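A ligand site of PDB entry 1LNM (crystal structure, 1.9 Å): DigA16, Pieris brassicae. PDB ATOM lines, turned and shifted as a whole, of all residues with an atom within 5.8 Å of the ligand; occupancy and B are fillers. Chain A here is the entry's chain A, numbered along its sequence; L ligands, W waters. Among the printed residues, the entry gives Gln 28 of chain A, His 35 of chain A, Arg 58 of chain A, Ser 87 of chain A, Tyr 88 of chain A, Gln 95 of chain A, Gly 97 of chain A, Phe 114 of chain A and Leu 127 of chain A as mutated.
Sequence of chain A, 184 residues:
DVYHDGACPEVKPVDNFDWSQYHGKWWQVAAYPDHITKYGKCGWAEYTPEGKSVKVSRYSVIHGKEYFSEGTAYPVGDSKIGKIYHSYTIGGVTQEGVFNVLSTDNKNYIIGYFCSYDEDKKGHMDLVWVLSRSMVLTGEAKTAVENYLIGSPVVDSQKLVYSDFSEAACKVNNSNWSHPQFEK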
ATOM      1  N   GLN A  28      19.814  28.437 -25.992  1.00  0.00           N
ATOM      2  CA  GLN A  28      20.773  29.424 -26.488  1.00  0.00           C
ATOM      3  C   GLN A  28      20.163  30.799 -26.681  1.00  0.00           C
ATOM      4  O   GLN A  28      19.629  31.099 -27.738  1.00  0.00           O
ATOM      5  CB  GLN A  28      21.376  28.916 -27.806  1.00  0.00           C
ATOM      6  CG  GLN A  28      22.708  29.525 -28.156  1.00  0.00           C
ATOM      7  CD  GLN A  28      23.275  28.927 -29.425  1.00  0.00           C
ATOM      8  OE1 GLN A  28      23.653  27.732 -29.425  1.00  0.00           O
ATOM      9  NE2 GLN A  28      23.295  29.747 -30.495  1.00  0.00           N
ATOM     10  N   HIS A  35      28.046  32.390 -35.399  1.00  0.00           N
ATOM     11  CA  HIS A  35      27.557  31.206 -34.735  1.00  0.00           C
ATOM     12  C   HIS A  35      26.128  30.889 -35.114  1.00  0.00           C
ATOM     13  O   HIS A  35      25.827  29.728 -35.401  1.00  0.00           O
ATOM     14  CB  HIS A  35      27.754  31.311 -33.221  1.00  0.00           C
ATOM     15  CG  HIS A  35      27.589  30.037 -32.459  1.00  0.00           C
ATOM     16  ND1 HIS A  35      26.384  29.585 -31.949  1.00  0.00           N
ATOM     17  CD2 HIS A  35      28.526  29.149 -32.038  1.00  0.00           C
ATOM     18  CE1 HIS A  35      26.579  28.463 -31.278  1.00  0.00           C
ATOM     19  NE2 HIS A  35      27.881  28.174 -31.310  1.00  0.00           N
ATOM     20  N   TYR A  39      25.670  27.263 -36.901  1.00  0.00           N
ATOM     21  CA  TYR A  39      25.013  26.269 -36.092  1.00  0.00           C
ATOM     22  C   TYR A  39      23.500  26.472 -35.851  1.00  0.00           C
ATOM     23  O   TYR A  39      22.900  25.677 -35.200  1.00  0.00           O
ATOM     24  CB  TYR A  39      25.828  26.215 -34.779  1.00  0.00           C
ATOM     25  CG  TYR A  39      27.310  26.051 -35.138  1.00  0.00           C
ATOM     26  CD1 TYR A  39      28.216  27.073 -34.888  1.00  0.00           C
ATOM     27  CD2 TYR A  39      27.769  24.892 -35.734  1.00  0.00           C
ATOM     28  CE1 TYR A  39      29.537  26.976 -35.260  1.00  0.00           C
ATOM     29  CE2 TYR A  39      29.126  24.750 -36.107  1.00  0.00           C
ATOM     30  CZ  TYR A  39      30.000  25.800 -35.854  1.00  0.00           C
ATOM     31  OH  TYR A  39      31.319  25.746 -36.210  1.00  0.00           O
ATOM     32  N   ALA A  45      19.156  22.787 -26.314  1.00  0.00           N
ATOM     33  CA  ALA A  45      19.840  21.498 -26.195  1.00  0.00           C
ATOM     34  C   ALA A  45      19.353  20.749 -24.972  1.00  0.00           C
ATOM     35  O   ALA A  45      19.046  21.372 -23.982  1.00  0.00           O
ATOM     36  CB  ALA A  45      21.358  21.733 -26.191  1.00  0.00           C
ATOM     37  N   TYR A  47      20.638  17.914 -22.373  1.00  0.00           N
ATOM     38  CA  TYR A  47      21.817  17.221 -21.847  1.00  0.00           C
ATOM     39  C   TYR A  47      21.435  16.075 -20.944  1.00  0.00           C
ATOM     40  O   TYR A  47      20.474  16.170 -20.150  1.00  0.00           O
ATOM     41  CB  TYR A  47      22.616  18.154 -20.977  1.00  0.00           C
ATOM     42  CG  TYR A  47      23.113  19.329 -21.693  1.00  0.00           C
ATOM     43  CD1 TYR A  47      22.581  20.563 -21.442  1.00  0.00           C
ATOM     44  CD2 TYR A  47      24.119  19.206 -22.644  1.00  0.00           C
ATOM     45  CE1 TYR A  47      23.058  21.695 -22.115  1.00  0.00           C
ATOM     46  CE2 TYR A  47      24.583  20.304 -23.315  1.00  0.00           C
ATOM     47  CZ  TYR A  47      24.060  21.558 -23.062  1.00  0.00           C
ATOM     48  OH  TYR A  47      24.558  22.650 -23.770  1.00  0.00           O
ATOM     49  N   VAL A  56      24.573  15.149 -25.678  1.00  0.00           N
ATOM     50  CA  VAL A  56      23.918  16.355 -26.140  1.00  0.00           C
ATOM     51  C   VAL A  56      23.041  16.024 -27.326  1.00  0.00           C
ATOM     52  O   VAL A  56      23.428  15.332 -28.273  1.00  0.00           O
ATOM     53  CB  VAL A  56      24.918  17.523 -26.465  1.00  0.00           C
ATOM     54  CG1 VAL A  56      24.191  18.866 -26.471  1.00  0.00           C
ATOM     55  CG2 VAL A  56      26.047  17.542 -25.530  1.00  0.00           C
ATOM     56  N   ARG A  58      20.606  18.445 -29.706  1.00  0.00           N
ATOM     57  CA  ARG A  58      20.362  19.833 -29.958  1.00  0.00           C
ATOM     58  C   ARG A  58      19.546  20.054 -31.227  1.00  0.00           C
ATOM     59  O   ARG A  58      19.677  19.410 -32.284  1.00  0.00           O
ATOM     60  CB  ARG A  58      21.731  20.481 -30.095  1.00  0.00           C
ATOM     61  CG  ARG A  58      21.658  21.947 -30.410  1.00  0.00           C
ATOM     62  CD  ARG A  58      23.043  22.478 -30.559  1.00  0.00           C
ATOM     63  NE  ARG A  58      23.038  23.931 -30.622  1.00  0.00           N
ATOM     64  CZ  ARG A  58      23.264  24.649 -31.722  1.00  0.00           C
ATOM     65  NH1 ARG A  58      23.468  24.089 -32.911  1.00  0.00           N
ATOM     66  NH2 ARG A  58      23.294  25.961 -31.611  1.00  0.00           N
ATOM     67  N   HIS A  86      34.116  18.724 -26.988  1.00  0.00           N
ATOM     68  CA  HIS A  86      32.791  18.430 -27.489  1.00  0.00           C
ATOM     69  C   HIS A  86      32.844  17.935 -28.903  1.00  0.00           C
ATOM     70  O   HIS A  86      33.518  18.565 -29.723  1.00  0.00           O
ATOM     71  CB  HIS A  86      32.123  19.749 -27.484  1.00  0.00           C
ATOM     72  CG  HIS A  86      30.656  19.771 -27.200  1.00  0.00           C
ATOM     73  ND1 HIS A  86      29.711  19.635 -28.187  1.00  0.00           N
ATOM     74  CD2 HIS A  86      29.982  20.092 -26.081  1.00  0.00           C
ATOM     75  CE1 HIS A  86      28.517  19.779 -27.666  1.00  0.00           C
ATOM     76  NE2 HIS A  86      28.651  20.075 -26.401  1.00  0.00           N
ATOM     77  N   SER A  87      32.146  16.843 -29.175  1.00  0.00           N
ATOM     78  CA  SER A  87      31.986  16.382 -30.566  1.00  0.00           C
ATOM     79  C   SER A  87      30.629  16.927 -31.036  1.00  0.00           C
ATOM     80  O   SER A  87      29.721  17.207 -30.233  1.00  0.00           O
ATOM     81  CB  SER A  87      31.950  14.876 -30.713  1.00  0.00           C
ATOM     82  OG  SER A  87      30.767  14.315 -30.152  1.00  0.00           O
ATOM     83  N   TYR A  88      30.472  17.011 -32.351  1.00  0.00           N
ATOM     84  CA  TYR A  88      29.300  17.629 -32.969  1.00  0.00           C
ATOM     85  C   TYR A  88      29.006  16.927 -34.277  1.00  0.00           C
ATOM     86  O   TYR A  88      29.783  17.082 -35.231  1.00  0.00           O
ATOM     87  CB  TYR A  88      29.592  19.119 -33.256  1.00  0.00           C
ATOM     88  CG  TYR A  88      28.472  19.912 -33.906  1.00  0.00           C
ATOM     89  CD1 TYR A  88      27.304  20.246 -33.196  1.00  0.00           C
ATOM     90  CD2 TYR A  88      28.584  20.369 -35.216  1.00  0.00           C
ATOM     91  CE1 TYR A  88      26.283  21.003 -33.771  1.00  0.00           C
ATOM     92  CE2 TYR A  88      27.555  21.140 -35.806  1.00  0.00           C
ATOM     93  CZ  TYR A  88      26.401  21.455 -35.097  1.00  0.00           C
ATOM     94  OH  TYR A  88      25.428  22.190 -35.717  1.00  0.00           O
ATOM     95  N   GLN A  95      32.381  16.710 -36.211  1.00  0.00           N
ATOM     96  CA  GLN A  95      33.441  17.685 -35.973  1.00  0.00           C
ATOM     97  C   GLN A  95      33.671  17.561 -34.492  1.00  0.00           C
ATOM     98  O   GLN A  95      32.766  17.061 -33.766  1.00  0.00           O
ATOM     99  CB  GLN A  95      33.016  19.102 -36.367  1.00  0.00           C
ATOM    100  CG  GLN A  95      33.078  19.422 -37.869  1.00  0.00           C
ATOM    101  CD  GLN A  95      32.323  20.702 -38.160  1.00  0.00           C
ATOM    102  OE1 GLN A  95      31.098  20.683 -38.279  1.00  0.00           O
ATOM    103  NE2 GLN A  95      33.047  21.813 -38.227  1.00  0.00           N
ATOM    104  N   GLU A  96      34.859  17.988 -34.067  1.00  0.00           N
ATOM    105  CA  GLU A  96      35.234  17.969 -32.669  1.00  0.00           C
ATOM    106  C   GLU A  96      36.169  19.100 -32.328  1.00  0.00           C
ATOM    107  O   GLU A  96      36.875  19.607 -33.187  1.00  0.00           O
ATOM    108  CB  GLU A  96      35.771  16.633 -32.209  1.00  0.00           C
ATOM    109  CG  GLU A  96      37.231  16.398 -32.541  1.00  0.00           C
ATOM    110  CD  GLU A  96      37.607  14.962 -32.302  1.00  0.00           C
ATOM    111  OE1 GLU A  96      38.595  14.563 -32.964  1.00  0.00           O
ATOM    112  OE2 GLU A  96      36.993  14.236 -31.480  1.00  0.00           O
ATOM    113  N   GLY A  97      36.153  19.452 -31.047  1.00  0.00           N
ATOM    114  CA  GLY A  97      36.942  20.551 -30.556  1.00  0.00           C
ATOM    115  C   GLY A  97      36.852  20.816 -29.096  1.00  0.00           C
ATOM    116  O   GLY A  97      36.066  20.210 -28.383  1.00  0.00           O
ATOM    117  N   VAL A  98      37.671  21.769 -28.705  1.00  0.00           N
ATOM    118  CA  VAL A  98      37.679  22.235 -27.318  1.00  0.00           C
ATOM    119  C   VAL A  98      37.316  23.690 -27.311  1.00  0.00           C
ATOM    120  O   VAL A  98      37.752  24.453 -28.165  1.00  0.00           O
ATOM    121  CB  VAL A  98      39.116  22.156 -26.770  1.00  0.00           C
ATOM    122  CG1 VAL A  98      39.215  22.660 -25.333  1.00  0.00           C
ATOM    123  CG2 VAL A  98      39.622  20.746 -26.967  1.00  0.00           C
ATOM    124  N   PHE A  99      36.479  24.028 -26.329  1.00  0.00           N
ATOM    125  CA  PHE A  99      36.157  25.421 -26.053  1.00  0.00           C
ATOM    126  C   PHE A  99      36.289  25.675 -24.557  1.00  0.00           C
ATOM    127  O   PHE A  99      36.507  24.787 -23.742  1.00  0.00           O
ATOM    128  CB  PHE A  99      34.762  25.757 -26.571  1.00  0.00           C
ATOM    129  CG  PHE A  99      33.625  25.212 -25.765  1.00  0.00           C
ATOM    130  CD1 PHE A  99      33.098  25.966 -24.716  1.00  0.00           C
ATOM    131  CD2 PHE A  99      33.019  23.970 -26.102  1.00  0.00           C
ATOM    132  CE1 PHE A  99      32.045  25.503 -23.926  1.00  0.00           C
ATOM    133  CE2 PHE A  99      31.985  23.510 -25.333  1.00  0.00           C
ATOM    134  CZ  PHE A  99      31.500  24.258 -24.227  1.00  0.00           C
ATOM    135  N   PHE A 114      35.078  30.065 -28.430  1.00  0.00           N
ATOM    136  CA  PHE A 114      36.029  29.374 -29.296  1.00  0.00           C
ATOM    137  C   PHE A 114      36.674  30.375 -30.230  1.00  0.00           C
ATOM    138  O   PHE A 114      36.002  31.262 -30.746  1.00  0.00           O
ATOM    139  CB  PHE A 114      35.204  28.325 -30.063  1.00  0.00           C
ATOM    140  CG  PHE A 114      35.985  27.557 -31.075  1.00  0.00           C
ATOM    141  CD1 PHE A 114      35.896  27.886 -32.425  1.00  0.00           C
ATOM    142  CD2 PHE A 114      36.797  26.509 -30.687  1.00  0.00           C
ATOM    143  CE1 PHE A 114      36.614  27.174 -33.371  1.00  0.00           C
ATOM    144  CE2 PHE A 114      37.542  25.810 -31.635  1.00  0.00           C
ATOM    145  CZ  PHE A 114      37.448  26.145 -32.970  1.00  0.00           C
ATOM    146  N   LEU A 127      33.934  32.945 -31.711  1.00  0.00           N
ATOM    147  CA  LEU A 127      32.546  32.517 -31.722  1.00  0.00           C
ATOM    148  C   LEU A 127      32.202  32.538 -30.280  1.00  0.00           C
ATOM    149  O   LEU A 127      32.953  32.051 -29.458  1.00  0.00           O
ATOM    150  CB  LEU A 127      32.356  31.081 -32.220  1.00  0.00           C
ATOM    151  CG  LEU A 127      32.516  30.824 -33.730  1.00  0.00           C
ATOM    152  CD1 LEU A 127      32.512  29.376 -34.263  1.00  0.00           C
ATOM    153  CD2 LEU A 127      31.536  31.704 -34.615  1.00  0.00           C
ATOM    154  N   TRP A 129      28.769  32.011 -27.713  1.00  0.00           N
ATOM    155  CA  TRP A 129      27.383  31.673 -27.458  1.00  0.00           C
ATOM    156  C   TRP A 129      27.023  31.619 -25.946  1.00  0.00           C
ATOM    157  O   TRP A 129      27.816  31.314 -25.057  1.00  0.00           O
ATOM    158  CB  TRP A 129      27.101  30.307 -28.115  1.00  0.00           C
ATOM    159  CG  TRP A 129      27.843  29.186 -27.552  1.00  0.00           C
ATOM    160  CD1 TRP A 129      27.385  28.289 -26.652  1.00  0.00           C
ATOM    161  CD2 TRP A 129      29.150  28.787 -27.885  1.00  0.00           C
ATOM    162  NE1 TRP A 129      28.341  27.335 -26.388  1.00  0.00           N
ATOM    163  CE2 TRP A 129      29.445  27.611 -27.149  1.00  0.00           C
ATOM    164  CE3 TRP A 129      30.104  29.271 -28.770  1.00  0.00           C
ATOM    165  CZ2 TRP A 129      30.672  26.957 -27.219  1.00  0.00           C
ATOM    166  CZ3 TRP A 129      31.354  28.589 -28.833  1.00  0.00           C
ATOM    167  CH2 TRP A 129      31.602  27.475 -28.074  1.00  0.00           C
ATOM    168  N   LEU A 131      24.306  30.155 -23.148  1.00  0.00           N
ATOM    169  CA  LEU A 131      23.229  29.251 -22.746  1.00  0.00           C
ATOM    170  C   LEU A 131      22.613  29.626 -21.392  1.00  0.00           C
ATOM    171  O   LEU A 131      23.312  30.089 -20.472  1.00  0.00           O
ATOM    172  CB  LEU A 131      23.725  27.819 -22.675  1.00  0.00           C
ATOM    173  CG  LEU A 131      24.333  27.290 -23.982  1.00  0.00           C
ATOM    174  CD1 LEU A 131      25.230  26.122 -23.699  1.00  0.00           C
ATOM    175  CD2 LEU A 131      23.222  26.946 -24.951  1.00  0.00           C
HETATM  176  O1  LIG L   1      24.531  23.630 -26.303  1.00  0.00           O
HETATM  177  C1  LIG L   1      25.205  23.778 -27.265  1.00  0.00           C
HETATM  178  C2  LIG L   1      25.903  22.854 -28.165  1.00  0.00           C
HETATM  179  O2  LIG L   1      25.428  25.082 -27.691  1.00  0.00           O
HETATM  180  C3  LIG L   1      26.278  25.035 -28.858  1.00  0.00           C
HETATM  181  C4  LIG L   1      26.532  23.601 -29.114  1.00  0.00           C
HETATM  182  C5  LIG L   1      27.506  23.243 -30.198  1.00  0.00           C
HETATM  183  C6  LIG L   1      27.224  24.163 -31.441  1.00  0.00           C
HETATM  184  C7  LIG L   1      28.976  23.370 -29.840  1.00  0.00           C
HETATM  185  C8  LIG L   1      29.712  22.114 -30.390  1.00  0.00           C
HETATM  186  C9  LIG L   1      31.228  22.229 -30.483  1.00  0.00           C
HETATM  187  C10 LIG L   1      29.226  23.507 -28.339  1.00  0.00           C
HETATM  188  C11 LIG L   1      29.468  24.572 -30.739  1.00  0.00           C
HETATM  189  C12 LIG L   1      28.636  24.411 -31.984  1.00  0.00           C
HETATM  190  O3  LIG L   1      28.937  25.805 -30.159  1.00  0.00           O
HETATM  191  C13 LIG L   1      31.003  24.720 -30.858  1.00  0.00           C
HETATM  192  C14 LIG L   1      31.368  25.968 -31.664  1.00  0.00           C
HETATM  193  C15 LIG L   1      31.689  23.410 -31.385  1.00  0.00           C
HETATM  194  C16 LIG L   1      33.230  23.612 -31.471  1.00  0.00           C
HETATM  195  C17 LIG L   1      33.867  22.332 -32.086  1.00  0.00           C
HETATM  196  C18 LIG L   1      33.953  23.727 -30.082  1.00  0.00           C
HETATM  197  C19 LIG L   1      33.510  24.767 -32.407  1.00  0.00           C
HETATM  198  C20 LIG L   1      32.881  26.092 -31.951  1.00  0.00           C
HETATM  199  C21 LIG L   1      33.013  24.465 -33.830  1.00  0.00           C
HETATM  200  C22 LIG L   1      33.589  23.174 -34.397  1.00  0.00           C
HETATM  201  C23 LIG L   1      33.296  22.014 -33.464  1.00  0.00           C
HETATM  202  O4  LIG L   1      35.038  23.342 -34.496  1.00  0.00           O
HETATM  203  O   HOH W   1      22.521  25.336 -28.213  1.00  0.00           O
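A ring nitrogen (NE2) of His 35 is in hydrogen-bond range of an oxygen (O3) of the ligand.
The side-chain hydroxyl of Tyr 47 lies within hydrogen-bond range of an oxygen (O1) of the ligand (2.7 Å).
The backbone carbonyl oxygen of Phe 114 sits at hydrogen-bond distance from the backbone NH of Leu 127, at 2.8 Å.
The guanidinium group (NH2) of Arg 58 is in hydrogen-bond range of the side-chain amide oxygen (OE1) of Gln 28, 2.8 Å away.
The side-chain amide nitrogen (NE2) of Gln 28 lies within hydrogen-bond range of a ring nitrogen (ND1) of His 35 (3.4 Å).
The backbone carbonyl oxygen (O) of Tyr 39 sits at hydrogen-bond distance from the guanidinium group (NH1) of Arg 58 (2.8 Å).
The backbone carbonyl oxygen (O) of Gly 97 lies within hydrogen-bond range of the backbone NH (N) of His 86, 2.8 Å away.
Gln 28 touches the ligand (OE1 to O2, 3.6 Å).
Tyr 39 touches the ligand.
Ala 45 touches the ligand.
Arg 58 touches the ligand.
His 86 touches the ligand.
Glu 96 touches the ligand.
Gly 97 touches the ligand (N to C17, 3.8 Å).
Phe 114 touches the ligand.
CE2 of Trp 129 touches O3 of the ligand, at 3.5 Å.
Leu 131 touches the ligand (CD1 to O1, 3.7 Å).
12 residues have an atom within 4 Å of the ligand: Gln 28, His 35, Tyr 39, Ala 45, Tyr 47, Arg 58, His 86, Glu 96, Gly 97, Phe 114, Trp 129 and Leu 131.
Along chain A the residues within 4 Å of the ligand span positions 28 to 131.
Water W1 lies within hydrogen-bond range of NE of Arg 58, OE1 of Gln 28 and O2 of the ligand.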
